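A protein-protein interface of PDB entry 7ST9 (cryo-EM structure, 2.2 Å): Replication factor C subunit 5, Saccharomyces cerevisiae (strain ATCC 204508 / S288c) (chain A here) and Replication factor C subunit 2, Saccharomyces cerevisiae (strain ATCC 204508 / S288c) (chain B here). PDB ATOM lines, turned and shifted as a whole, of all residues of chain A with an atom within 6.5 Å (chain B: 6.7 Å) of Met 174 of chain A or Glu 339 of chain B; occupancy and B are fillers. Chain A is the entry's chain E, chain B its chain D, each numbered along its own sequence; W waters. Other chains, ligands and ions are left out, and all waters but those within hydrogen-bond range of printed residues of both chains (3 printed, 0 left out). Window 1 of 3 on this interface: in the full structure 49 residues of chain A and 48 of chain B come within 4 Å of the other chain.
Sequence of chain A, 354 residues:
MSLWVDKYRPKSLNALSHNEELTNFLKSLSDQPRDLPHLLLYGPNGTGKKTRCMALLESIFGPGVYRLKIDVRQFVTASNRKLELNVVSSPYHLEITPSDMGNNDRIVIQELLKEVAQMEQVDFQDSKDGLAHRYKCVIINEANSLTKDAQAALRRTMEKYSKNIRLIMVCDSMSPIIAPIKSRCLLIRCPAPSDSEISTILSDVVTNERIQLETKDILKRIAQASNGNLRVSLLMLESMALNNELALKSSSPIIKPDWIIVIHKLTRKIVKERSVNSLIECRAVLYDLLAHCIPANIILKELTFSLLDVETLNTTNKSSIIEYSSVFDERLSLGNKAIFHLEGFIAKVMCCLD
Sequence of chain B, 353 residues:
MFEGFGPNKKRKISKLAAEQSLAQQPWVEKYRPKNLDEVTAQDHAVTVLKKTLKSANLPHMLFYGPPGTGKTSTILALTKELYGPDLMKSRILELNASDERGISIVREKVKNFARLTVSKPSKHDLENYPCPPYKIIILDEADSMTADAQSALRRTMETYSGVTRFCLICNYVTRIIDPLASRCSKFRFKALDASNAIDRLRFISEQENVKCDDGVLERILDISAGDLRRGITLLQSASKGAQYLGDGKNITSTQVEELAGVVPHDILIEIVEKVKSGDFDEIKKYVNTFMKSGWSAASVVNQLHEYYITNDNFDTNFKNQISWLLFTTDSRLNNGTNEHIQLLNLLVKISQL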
ATOM      1  N   LEU A  40     -34.276  30.106 -11.208  1.00  0.00           N
ATOM      2  CA  LEU A  40     -33.976  28.683 -11.049  1.00  0.00           C
ATOM      3  C   LEU A  40     -33.343  28.512  -9.671  1.00  0.00           C
ATOM      4  O   LEU A  40     -32.175  28.852  -9.470  1.00  0.00           O
ATOM      5  CB  LEU A  40     -33.057  28.178 -12.158  1.00  0.00           C
ATOM      6  CG  LEU A  40     -32.496  26.761 -11.993  1.00  0.00           C
ATOM      7  CD1 LEU A  40     -33.589  25.772 -11.617  1.00  0.00           C
ATOM      8  CD2 LEU A  40     -31.789  26.314 -13.262  1.00  0.00           C
ATOM      9  N   LEU A  41     -34.125  28.008  -8.722  1.00  0.00           N
ATOM     10  CA  LEU A  41     -33.649  27.749  -7.371  1.00  0.00           C
ATOM     11  C   LEU A  41     -33.145  26.313  -7.299  1.00  0.00           C
ATOM     12  O   LEU A  41     -33.889  25.376  -7.605  1.00  0.00           O
ATOM     13  CB  LEU A  41     -34.761  27.977  -6.348  1.00  0.00           C
ATOM     14  CG  LEU A  41     -35.133  29.428  -6.042  1.00  0.00           C
ATOM     15  CD1 LEU A  41     -35.980  30.019  -7.158  1.00  0.00           C
ATOM     16  CD2 LEU A  41     -35.861  29.516  -4.710  1.00  0.00           C
ATOM     17  N   TYR A  42     -31.890  26.143  -6.899  1.00  0.00           N
ATOM     18  CA  TYR A  42     -31.291  24.824  -6.768  1.00  0.00           C
ATOM     19  C   TYR A  42     -30.755  24.638  -5.357  1.00  0.00           C
ATOM     20  O   TYR A  42     -30.156  25.553  -4.780  1.00  0.00           O
ATOM     21  CB  TYR A  42     -30.173  24.610  -7.798  1.00  0.00           C
ATOM     22  CG  TYR A  42     -28.981  25.524  -7.645  1.00  0.00           C
ATOM     23  CD1 TYR A  42     -29.009  26.820  -8.139  1.00  0.00           C
ATOM     24  CD2 TYR A  42     -27.821  25.085  -7.021  1.00  0.00           C
ATOM     25  CE1 TYR A  42     -27.920  27.656  -8.009  1.00  0.00           C
ATOM     26  CE2 TYR A  42     -26.727  25.914  -6.885  1.00  0.00           C
ATOM     27  CZ  TYR A  42     -26.781  27.198  -7.381  1.00  0.00           C
ATOM     28  OH  TYR A  42     -25.693  28.029  -7.248  1.00  0.00           O
ATOM     29  N   ASN A 144     -35.091  19.324 -12.824  1.00  0.00           N
ATOM     30  CA  ASN A 144     -33.974  18.483 -13.235  1.00  0.00           C
ATOM     31  C   ASN A 144     -34.415  17.136 -13.793  1.00  0.00           C
ATOM     32  O   ASN A 144     -33.592  16.442 -14.400  1.00  0.00           O
ATOM     33  CB  ASN A 144     -33.023  18.265 -12.055  1.00  0.00           C
ATOM     34  CG  ASN A 144     -33.709  17.640 -10.858  1.00  0.00           C
ATOM     35  OD1 ASN A 144     -34.876  17.917 -10.581  1.00  0.00           O
ATOM     36  ND2 ASN A 144     -32.985  16.793 -10.138  1.00  0.00           N
ATOM     37  N   CYS A 171     -35.018  22.796  -8.311  1.00  0.00           N
ATOM     38  CA  CYS A 171     -34.293  21.554  -8.539  1.00  0.00           C
ATOM     39  C   CYS A 171     -33.359  21.253  -7.374  1.00  0.00           C
ATOM     40  O   CYS A 171     -32.972  22.136  -6.600  1.00  0.00           O
ATOM     41  CB  CYS A 171     -33.500  21.611  -9.853  1.00  0.00           C
ATOM     42  SG  CYS A 171     -32.025  22.646  -9.792  1.00  0.00           S
ATOM     43  N   ASP A 172     -32.996  19.974  -7.266  1.00  0.00           N
ATOM     44  CA  ASP A 172     -32.033  19.530  -6.270  1.00  0.00           C
ATOM     45  C   ASP A 172     -30.606  19.516  -6.797  1.00  0.00           C
ATOM     46  O   ASP A 172     -29.665  19.622  -6.002  1.00  0.00           O
ATOM     47  CB  ASP A 172     -32.401  18.132  -5.758  1.00  0.00           C
ATOM     48  CG  ASP A 172     -32.662  17.145  -6.880  1.00  0.00           C
ATOM     49  OD1 ASP A 172     -31.916  17.167  -7.880  1.00  0.00           O
ATOM     50  OD2 ASP A 172     -33.616  16.347  -6.761  1.00  0.00           O
ATOM     51  N   SER A 173     -30.425  19.389  -8.109  1.00  0.00           N
ATOM     52  CA  SER A 173     -29.105  19.434  -8.719  1.00  0.00           C
ATOM     53  C   SER A 173     -29.237  20.012 -10.119  1.00  0.00           C
ATOM     54  O   SER A 173     -30.200  19.715 -10.830  1.00  0.00           O
ATOM     55  CB  SER A 173     -28.463  18.042  -8.777  1.00  0.00           C
ATOM     56  OG  SER A 173     -29.277  17.136  -9.501  1.00  0.00           O
ATOM     57  N   MET A 174     -28.268  20.836 -10.505  1.00  0.00           N
ATOM     58  CA  MET A 174     -28.262  21.466 -11.818  1.00  0.00           C
ATOM     59  C   MET A 174     -27.518  20.648 -12.866  1.00  0.00           C
ATOM     60  O   MET A 174     -27.486  21.048 -14.034  1.00  0.00           O
ATOM     61  CB  MET A 174     -27.641  22.864 -11.722  1.00  0.00           C
ATOM     62  CG  MET A 174     -28.589  23.920 -11.172  1.00  0.00           C
ATOM     63  SD  MET A 174     -27.991  25.603 -11.410  1.00  0.00           S
ATOM     64  CE  MET A 174     -26.424  25.538 -10.547  1.00  0.00           C
ATOM     65  N   SER A 175     -26.923  19.519 -12.482  1.00  0.00           N
ATOM     66  CA  SER A 175     -26.196  18.707 -13.454  1.00  0.00           C
ATOM     67  C   SER A 175     -27.065  18.277 -14.630  1.00  0.00           C
ATOM     68  O   SER A 175     -26.577  18.331 -15.772  1.00  0.00           O
ATOM     69  CB  SER A 175     -25.580  17.488 -12.752  1.00  0.00           C
ATOM     70  OG  SER A 175     -26.291  16.301 -13.051  1.00  0.00           O
ATOM     71  N   PRO A 176     -28.316  17.847 -14.446  1.00  0.00           N
ATOM     72  CA  PRO A 176     -29.142  17.445 -15.592  1.00  0.00           C
ATOM     73  C   PRO A 176     -29.765  18.602 -16.364  1.00  0.00           C
ATOM     74  O   PRO A 176     -30.451  18.349 -17.361  1.00  0.00           O
ATOM     75  CB  PRO A 176     -30.236  16.572 -14.945  1.00  0.00           C
ATOM     76  CG  PRO A 176     -29.823  16.379 -13.509  1.00  0.00           C
ATOM     77  CD  PRO A 176     -28.993  17.563 -13.172  1.00  0.00           C
ATOM     78  N   ILE A 177     -29.565  19.847 -15.943  1.00  0.00           N
ATOM     79  CA  ILE A 177     -30.130  20.992 -16.653  1.00  0.00           C
ATOM     80  C   ILE A 177     -29.213  21.356 -17.814  1.00  0.00           C
ATOM     81  O   ILE A 177     -28.011  21.575 -17.626  1.00  0.00           O
ATOM     82  CB  ILE A 177     -30.319  22.188 -15.704  1.00  0.00           C
ATOM     83  CG1 ILE A 177     -31.116  21.782 -14.458  1.00  0.00           C
ATOM     84  CG2 ILE A 177     -31.005  23.338 -16.432  1.00  0.00           C
ATOM     85  CD1 ILE A 177     -32.557  21.412 -14.731  1.00  0.00           C
ATOM     86  N   ILE A 178     -29.780  21.432 -19.020  1.00  0.00           N
ATOM     87  CA  ILE A 178     -28.980  21.755 -20.195  1.00  0.00           C
ATOM     88  C   ILE A 178     -28.476  23.191 -20.099  1.00  0.00           C
ATOM     89  O   ILE A 178     -29.112  24.063 -19.492  1.00  0.00           O
ATOM     90  CB  ILE A 178     -29.783  21.530 -21.491  1.00  0.00           C
ATOM     91  CG1 ILE A 178     -30.982  22.483 -21.567  1.00  0.00           C
ATOM     92  CG2 ILE A 178     -30.246  20.083 -21.581  1.00  0.00           C
ATOM     93  CD1 ILE A 178     -31.766  22.368 -22.859  1.00  0.00           C
ATOM     94  N   LYS A 182     -29.946  26.919 -18.284  1.00  0.00           N
ATOM     95  CA  LYS A 182     -29.234  27.633 -17.229  1.00  0.00           C
ATOM     96  C   LYS A 182     -28.869  29.044 -17.666  1.00  0.00           C
ATOM     97  O   LYS A 182     -28.840  29.963 -16.839  1.00  0.00           O
ATOM     98  CB  LYS A 182     -27.977  26.862 -16.826  1.00  0.00           C
ATOM     99  CG  LYS A 182     -28.229  25.738 -15.836  1.00  0.00           C
ATOM    100  CD  LYS A 182     -27.138  24.679 -15.894  1.00  0.00           C
ATOM    101  CE  LYS A 182     -25.777  25.246 -15.524  1.00  0.00           C
ATOM    102  NZ  LYS A 182     -25.764  25.848 -14.163  1.00  0.00           N
ATOM    103  N   LEU A 187     -29.856  32.038 -11.368  1.00  0.00           N
ATOM    104  CA  LEU A 187     -29.598  30.874 -10.530  1.00  0.00           C
ATOM    105  C   LEU A 187     -29.500  31.298  -9.071  1.00  0.00           C
ATOM    106  O   LEU A 187     -28.726  32.198  -8.730  1.00  0.00           O
ATOM    107  CB  LEU A 187     -28.310  30.171 -10.965  1.00  0.00           C
ATOM    108  CG  LEU A 187     -28.128  29.979 -12.472  1.00  0.00           C
ATOM    109  CD1 LEU A 187     -26.765  29.374 -12.774  1.00  0.00           C
ATOM    110  CD2 LEU A 187     -29.240  29.116 -13.046  1.00  0.00           C
ATOM    111  N   ILE A 188     -30.282  30.647  -8.216  1.00  0.00           N
ATOM    112  CA  ILE A 188     -30.338  30.959  -6.793  1.00  0.00           C
ATOM    113  C   ILE A 188     -29.993  29.695  -6.018  1.00  0.00           C
ATOM    114  O   ILE A 188     -30.709  28.688  -6.106  1.00  0.00           O
ATOM    115  CB  ILE A 188     -31.718  31.498  -6.381  1.00  0.00           C
ATOM    116  CG1 ILE A 188     -32.027  32.795  -7.136  1.00  0.00           C
ATOM    117  CG2 ILE A 188     -31.771  31.729  -4.875  1.00  0.00           C
ATOM    118  CD1 ILE A 188     -33.479  33.216  -7.068  1.00  0.00           C
ATOM    119  N   ASP A 329     -23.129   4.952 -11.629  1.00  0.00           N
ATOM    120  CA  ASP A 329     -24.046   6.084 -11.674  1.00  0.00           C
ATOM    121  C   ASP A 329     -24.108   6.670 -13.078  1.00  0.00           C
ATOM    122  O   ASP A 329     -25.196   6.985 -13.581  1.00  0.00           O
ATOM    123  CB  ASP A 329     -23.615   7.140 -10.657  1.00  0.00           C
ATOM    124  CG  ASP A 329     -24.483   8.381 -10.699  1.00  0.00           C
ATOM    125  OD1 ASP A 329     -25.720   8.250 -10.589  1.00  0.00           O
ATOM    126  OD2 ASP A 329     -23.927   9.488 -10.831  1.00  0.00           O
ATOM    127  N   VAL B 287     -16.699  16.444   2.461  1.00  0.00           N
ATOM    128  CA  VAL B 287     -17.550  16.534   1.280  1.00  0.00           C
ATOM    129  C   VAL B 287     -19.018  16.425   1.672  1.00  0.00           C
ATOM    130  O   VAL B 287     -19.876  17.123   1.115  1.00  0.00           O
ATOM    131  CB  VAL B 287     -17.152  15.455   0.256  1.00  0.00           C
ATOM    132  CG1 VAL B 287     -18.168  15.391  -0.873  1.00  0.00           C
ATOM    133  CG2 VAL B 287     -15.765  15.734  -0.294  1.00  0.00           C
ATOM    134  N   MET B 291     -21.533  19.486   0.627  1.00  0.00           N
ATOM    135  CA  MET B 291     -22.677  19.371  -0.272  1.00  0.00           C
ATOM    136  C   MET B 291     -23.974  19.872   0.350  1.00  0.00           C
ATOM    137  O   MET B 291     -24.953  20.063  -0.378  1.00  0.00           O
ATOM    138  CB  MET B 291     -22.851  17.922  -0.732  1.00  0.00           C
ATOM    139  CG  MET B 291     -21.606  17.314  -1.376  1.00  0.00           C
ATOM    140  SD  MET B 291     -21.342  17.754  -3.111  1.00  0.00           S
ATOM    141  CE  MET B 291     -22.969  17.543  -3.829  1.00  0.00           C
ATOM    142  N   GLY B 294     -25.100  23.264  -1.111  1.00  0.00           N
ATOM    143  CA  GLY B 294     -25.746  23.247  -2.406  1.00  0.00           C
ATOM    144  C   GLY B 294     -24.908  23.748  -3.559  1.00  0.00           C
ATOM    145  O   GLY B 294     -25.462  24.025  -4.628  1.00  0.00           O
ATOM    146  N   TRP B 295     -23.594  23.874  -3.382  1.00  0.00           N
ATOM    147  CA  TRP B 295     -22.734  24.329  -4.467  1.00  0.00           C
ATOM    148  C   TRP B 295     -22.849  23.396  -5.666  1.00  0.00           C
ATOM    149  O   TRP B 295     -22.874  22.171  -5.523  1.00  0.00           O
ATOM    150  CB  TRP B 295     -21.279  24.394  -4.000  1.00  0.00           C
ATOM    151  CG  TRP B 295     -21.057  25.276  -2.812  1.00  0.00           C
ATOM    152  CD1 TRP B 295     -20.803  24.877  -1.534  1.00  0.00           C
ATOM    153  CD2 TRP B 295     -21.062  26.707  -2.791  1.00  0.00           C
ATOM    154  NE1 TRP B 295     -20.650  25.970  -0.716  1.00  0.00           N
ATOM    155  CE2 TRP B 295     -20.806  27.106  -1.465  1.00  0.00           C
ATOM    156  CE3 TRP B 295     -21.261  27.691  -3.765  1.00  0.00           C
ATOM    157  CZ2 TRP B 295     -20.743  28.445  -1.089  1.00  0.00           C
ATOM    158  CZ3 TRP B 295     -21.198  29.018  -3.389  1.00  0.00           C
ATOM    159  CH2 TRP B 295     -20.942  29.384  -2.063  1.00  0.00           C
ATOM    160  N   SER B 296     -22.922  23.983  -6.857  1.00  0.00           N
ATOM    161  CA  SER B 296     -22.978  23.189  -8.078  1.00  0.00           C
ATOM    162  C   SER B 296     -21.625  22.535  -8.333  1.00  0.00           C
ATOM    163  O   SER B 296     -20.582  23.190  -8.256  1.00  0.00           O
ATOM    164  CB  SER B 296     -23.380  24.063  -9.264  1.00  0.00           C
ATOM    165  OG  SER B 296     -22.400  25.053  -9.527  1.00  0.00           O
ATOM    166  N   ALA B 297     -21.646  21.236  -8.642  1.00  0.00           N
ATOM    167  CA  ALA B 297     -20.400  20.500  -8.824  1.00  0.00           C
ATOM    168  C   ALA B 297     -19.591  21.036  -9.997  1.00  0.00           C
ATOM    169  O   ALA B 297     -18.356  21.004  -9.962  1.00  0.00           O
ATOM    170  CB  ALA B 297     -20.695  19.014  -9.024  1.00  0.00           C
ATOM    171  N   ALA B 298     -20.260  21.523 -11.044  1.00  0.00           N
ATOM    172  CA  ALA B 298     -19.539  22.037 -12.204  1.00  0.00           C
ATOM    173  C   ALA B 298     -18.647  23.212 -11.823  1.00  0.00           C
ATOM    174  O   ALA B 298     -17.487  23.285 -12.249  1.00  0.00           O
ATOM    175  CB  ALA B 298     -20.528  22.447 -13.293  1.00  0.00           C
ATOM    176  N   LEU B 333     -20.320  14.518 -15.279  1.00  0.00           N
ATOM    177  CA  LEU B 333     -21.290  15.493 -14.793  1.00  0.00           C
ATOM    178  C   LEU B 333     -22.172  16.000 -15.926  1.00  0.00           C
ATOM    179  O   LEU B 333     -23.390  16.138 -15.761  1.00  0.00           O
ATOM    180  CB  LEU B 333     -20.569  16.656 -14.113  1.00  0.00           C
ATOM    181  CG  LEU B 333     -20.076  16.388 -12.689  1.00  0.00           C
ATOM    182  CD1 LEU B 333     -19.117  17.479 -12.247  1.00  0.00           C
ATOM    183  CD2 LEU B 333     -21.247  16.276 -11.723  1.00  0.00           C
ATOM    184  N   THR B 337     -25.125  13.275 -13.786  1.00  0.00           N
ATOM    185  CA  THR B 337     -24.891  12.288 -12.742  1.00  0.00           C
ATOM    186  C   THR B 337     -25.020  12.927 -11.363  1.00  0.00           C
ATOM    187  O   THR B 337     -25.094  14.149 -11.216  1.00  0.00           O
ATOM    188  CB  THR B 337     -23.501  11.656 -12.902  1.00  0.00           C
ATOM    189  OG1 THR B 337     -22.564  12.654 -13.323  1.00  0.00           O
ATOM    190  CG2 THR B 337     -23.540  10.532 -13.924  1.00  0.00           C
ATOM    191  N   ASN B 338     -25.045  12.069 -10.345  1.00  0.00           N
ATOM    192  CA  ASN B 338     -25.111  12.535  -8.965  1.00  0.00           C
ATOM    193  C   ASN B 338     -23.861  13.332  -8.619  1.00  0.00           C
ATOM    194  O   ASN B 338     -22.740  12.826  -8.727  1.00  0.00           O
ATOM    195  CB  ASN B 338     -25.266  11.344  -8.021  1.00  0.00           C
ATOM    196  CG  ASN B 338     -25.443  11.763  -6.576  1.00  0.00           C
ATOM    197  OD1 ASN B 338     -24.473  11.885  -5.829  1.00  0.00           O
ATOM    198  ND2 ASN B 338     -26.688  11.987  -6.172  1.00  0.00           N
ATOM    199  N   GLU B 339     -24.057  14.579  -8.189  1.00  0.00           N
ATOM    200  CA  GLU B 339     -22.926  15.471  -7.950  1.00  0.00           C
ATOM    201  C   GLU B 339     -22.066  14.991  -6.786  1.00  0.00           C
ATOM    202  O   GLU B 339     -20.833  15.053  -6.853  1.00  0.00           O
ATOM    203  CB  GLU B 339     -23.431  16.890  -7.696  1.00  0.00           C
ATOM    204  CG  GLU B 339     -23.942  17.583  -8.949  1.00  0.00           C
ATOM    205  CD  GLU B 339     -24.610  18.913  -8.658  1.00  0.00           C
ATOM    206  OE1 GLU B 339     -24.318  19.514  -7.602  1.00  0.00           O
ATOM    207  OE2 GLU B 339     -25.433  19.356  -9.487  1.00  0.00           O
ATOM    208  N   HIS B 340     -22.696  14.516  -5.709  1.00  0.00           N
ATOM    209  CA  HIS B 340     -21.941  14.099  -4.530  1.00  0.00           C
ATOM    210  C   HIS B 340     -20.981  12.963  -4.865  1.00  0.00           C
ATOM    211  O   HIS B 340     -19.794  13.011  -4.514  1.00  0.00           O
ATOM    212  CB  HIS B 340     -22.913  13.682  -3.423  1.00  0.00           C
ATOM    213  CG  HIS B 340     -22.279  13.540  -2.075  1.00  0.00           C
ATOM    214  ND1 HIS B 340     -23.016  13.406  -0.918  1.00  0.00           N
ATOM    215  CD2 HIS B 340     -20.979  13.509  -1.697  1.00  0.00           C
ATOM    216  CE1 HIS B 340     -22.199  13.301   0.114  1.00  0.00           C
ATOM    217  NE2 HIS B 340     -20.957  13.359  -0.332  1.00  0.00           N
ATOM    218  N   ILE B 341     -21.478  11.933  -5.553  1.00  0.00           N
ATOM    219  CA  ILE B 341     -20.649  10.770  -5.864  1.00  0.00           C
ATOM    220  C   ILE B 341     -19.476  11.176  -6.747  1.00  0.00           C
ATOM    221  O   ILE B 341     -18.323  10.812  -6.488  1.00  0.00           O
ATOM    222  CB  ILE B 341     -21.498   9.671  -6.529  1.00  0.00           C
ATOM    223  CG1 ILE B 341     -22.431   9.023  -5.504  1.00  0.00           C
ATOM    224  CG2 ILE B 341     -20.606   8.616  -7.173  1.00  0.00           C
ATOM    225  CD1 ILE B 341     -23.621   8.325  -6.123  1.00  0.00           C
ATOM    226  N   GLN B 342     -19.757  11.932  -7.813  1.00  0.00           N
ATOM    227  CA  GLN B 342     -18.701  12.316  -8.742  1.00  0.00           C
ATOM    228  C   GLN B 342     -17.657  13.188  -8.058  1.00  0.00           C
ATOM    229  O   GLN B 342     -16.450  13.000  -8.261  1.00  0.00           O
ATOM    230  CB  GLN B 342     -19.301  13.042  -9.947  1.00  0.00           C
ATOM    231  CG  GLN B 342     -20.328  12.224 -10.719  1.00  0.00           C
ATOM    232  CD  GLN B 342     -19.747  10.951 -11.304  1.00  0.00           C
ATOM    233  OE1 GLN B 342     -18.539  10.840 -11.503  1.00  0.00           O
ATOM    234  NE2 GLN B 342     -20.610   9.981 -11.584  1.00  0.00           N
ATOM    235  N   LEU B 343     -18.099  14.148  -7.241  1.00  0.00           N
ATOM    236  CA  LEU B 343     -17.155  15.017  -6.549  1.00  0.00           C
ATOM    237  C   LEU B 343     -16.282  14.224  -5.585  1.00  0.00           C
ATOM    238  O   LEU B 343     -15.062  14.429  -5.528  1.00  0.00           O
ATOM    239  CB  LEU B 343     -17.906  16.124  -5.807  1.00  0.00           C
ATOM    240  CG  LEU B 343     -17.033  17.112  -5.029  1.00  0.00           C
ATOM    241  CD1 LEU B 343     -16.000  17.761  -5.941  1.00  0.00           C
ATOM    242  CD2 LEU B 343     -17.893  18.168  -4.352  1.00  0.00           C
ATOM    243  N   LEU B 344     -16.885  13.314  -4.815  1.00  0.00           N
ATOM    244  CA  LEU B 344     -16.099  12.509  -3.886  1.00  0.00           C
ATOM    245  C   LEU B 344     -15.094  11.640  -4.630  1.00  0.00           C
ATOM    246  O   LEU B 344     -13.937  11.517  -4.211  1.00  0.00           O
ATOM    247  CB  LEU B 344     -17.024  11.650  -3.023  1.00  0.00           C
ATOM    248  CG  LEU B 344     -16.338  10.734  -2.005  1.00  0.00           C
ATOM    249  CD1 LEU B 344     -15.424  11.526  -1.083  1.00  0.00           C
ATOM    250  CD2 LEU B 344     -17.373   9.963  -1.202  1.00  0.00           C
HETATM  251  O   HOH W   1     -26.651  18.091  -6.115  1.00  0.00           O
HETATM  252  O   HOH W   2     -26.273  21.681  -8.677  1.00  0.00           O
HETATM  253  O   HOH W   3     -27.744  14.715 -11.239  1.00  0.00           O
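Printed residues of chain B within 4 Å of Met 174 of chain A: Ser 296 and Glu 339.
Glu 339 of chain B touches just these residues of chain A: Ser 173 (3.4 Å), Met 174 (3.4 Å) and Ser 175 (3.3 Å).
Of the printed residues of chain A, Ser 296 of chain B touches Met 174.
Of the printed residues of chain B, Tyr 42 of chain A touches Gly 294.
Printed residues of chain B within 4 Å of Ser 175 of chain A: Leu 333, Thr 337 and Glu 339.
Printed residues of chain B within 4 Å of Asp 329 of chain A: Thr 337 (3.0 Å), Asn 338 (2.9 Å) and Gln 342 (3.4 Å).
Met 291 of chain B touches none of the printed residues of chain A.
The nearest residue of chain B that does not touch Met 174 of chain A is Gly 294 of chain B (6.2 Å).
The backbone NH (N) of Ala 297 of chain B sits at hydrogen-bond distance from the side-chain carboxylate (OE1) of Glu 339 of chain B.
The side-chain amide oxygen (OD1) of Asn 338 of chain B lies within hydrogen-bond range of the backbone NH (N) of Ile 341 of chain B (3.0 Å).
SG of Cys 171 of chain A lies within hydrogen-bond range of O of Ser 173 of chain A (3.6 Å).
The side-chain amino group (NZ) of Lys 182 of chain A lies within hydrogen-bond range of the side-chain sulfur (SD) of Met 174 of chain A, 3.5 Å away.
OD1 of Asp 172 of chain A lies within hydrogen-bond range of OG of Ser 173 of chain A, 3.1 Å away.
The backbone NH (N) of Tyr 42 of chain A is in hydrogen-bond range of the backbone carbonyl oxygen (O) of Ile 188 of chain A, 2.9 Å away.
O of Thr 337 of chain B sits at hydrogen-bond distance from OG of Ser 175 of chain A (3.1 Å).
The side-chain carboxylate (OD2) of Asp 329 of chain A is in hydrogen-bond range of the side-chain amide nitrogen (NE2) of Gln 342 of chain B (3.4 Å).
OE2 of Glu 339 of chain B is in hydrogen-bond range of N of Ser 175 of chain A (3.3 Å).
The backbone NH (N) of Asn 338 of chain B lies within hydrogen-bond range of the side-chain carboxylate (OD2) of Asp 329 of chain A, 2.9 Å away.
The backbone NH (N) of Met 174 of chain A sits at hydrogen-bond distance from the side-chain carboxylate (OE2) of Glu 339 of chain B, at 3.4 Å.
Hydrophobic or aromatic side chains of chain A within 4 Å of the printed part of chain B: Tyr 42 and Met 174.
Among the printed residues, 10 pairs touch across the chains.
Among the printed residues, no Asp or Glu carboxylate lies within 4 Å of a Lys or Arg side-chain nitrogen of the other chain.
Water W2 lies within hydrogen-bond range of OE2 of Glu 339 of chain B (2.6 Å) and N of Met 174 of chain A (2.8 Å).
Water W3 lies within hydrogen-bond range of O of Thr 337 of chain B (2.7 Å), OG of Ser 175 of chain A (2.8 Å) and OG of Ser 173 of chain A (3.4 Å).
Water W1 lies within hydrogen-bond range of the side-chain carboxylate of Glu 339 of chain B (3.1 Å) and the backbone carbonyl oxygen of Asp 172 of chain A (3.4 Å).
Gly 294 of chain B touches Tyr 42 of chain A (O to CE2, 3.2 Å).
OE2 of Glu 339 of chain B touches CB of Ser 173 of chain A, at 3.4 Å.
Met 174 of chain A touches Ser 296 of chain B.
O of Ser 175 of chain A touches O of Leu 333 of chain B, at 3.9 Å.
Asp 329 of chain A touches Thr 337 of chain B.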
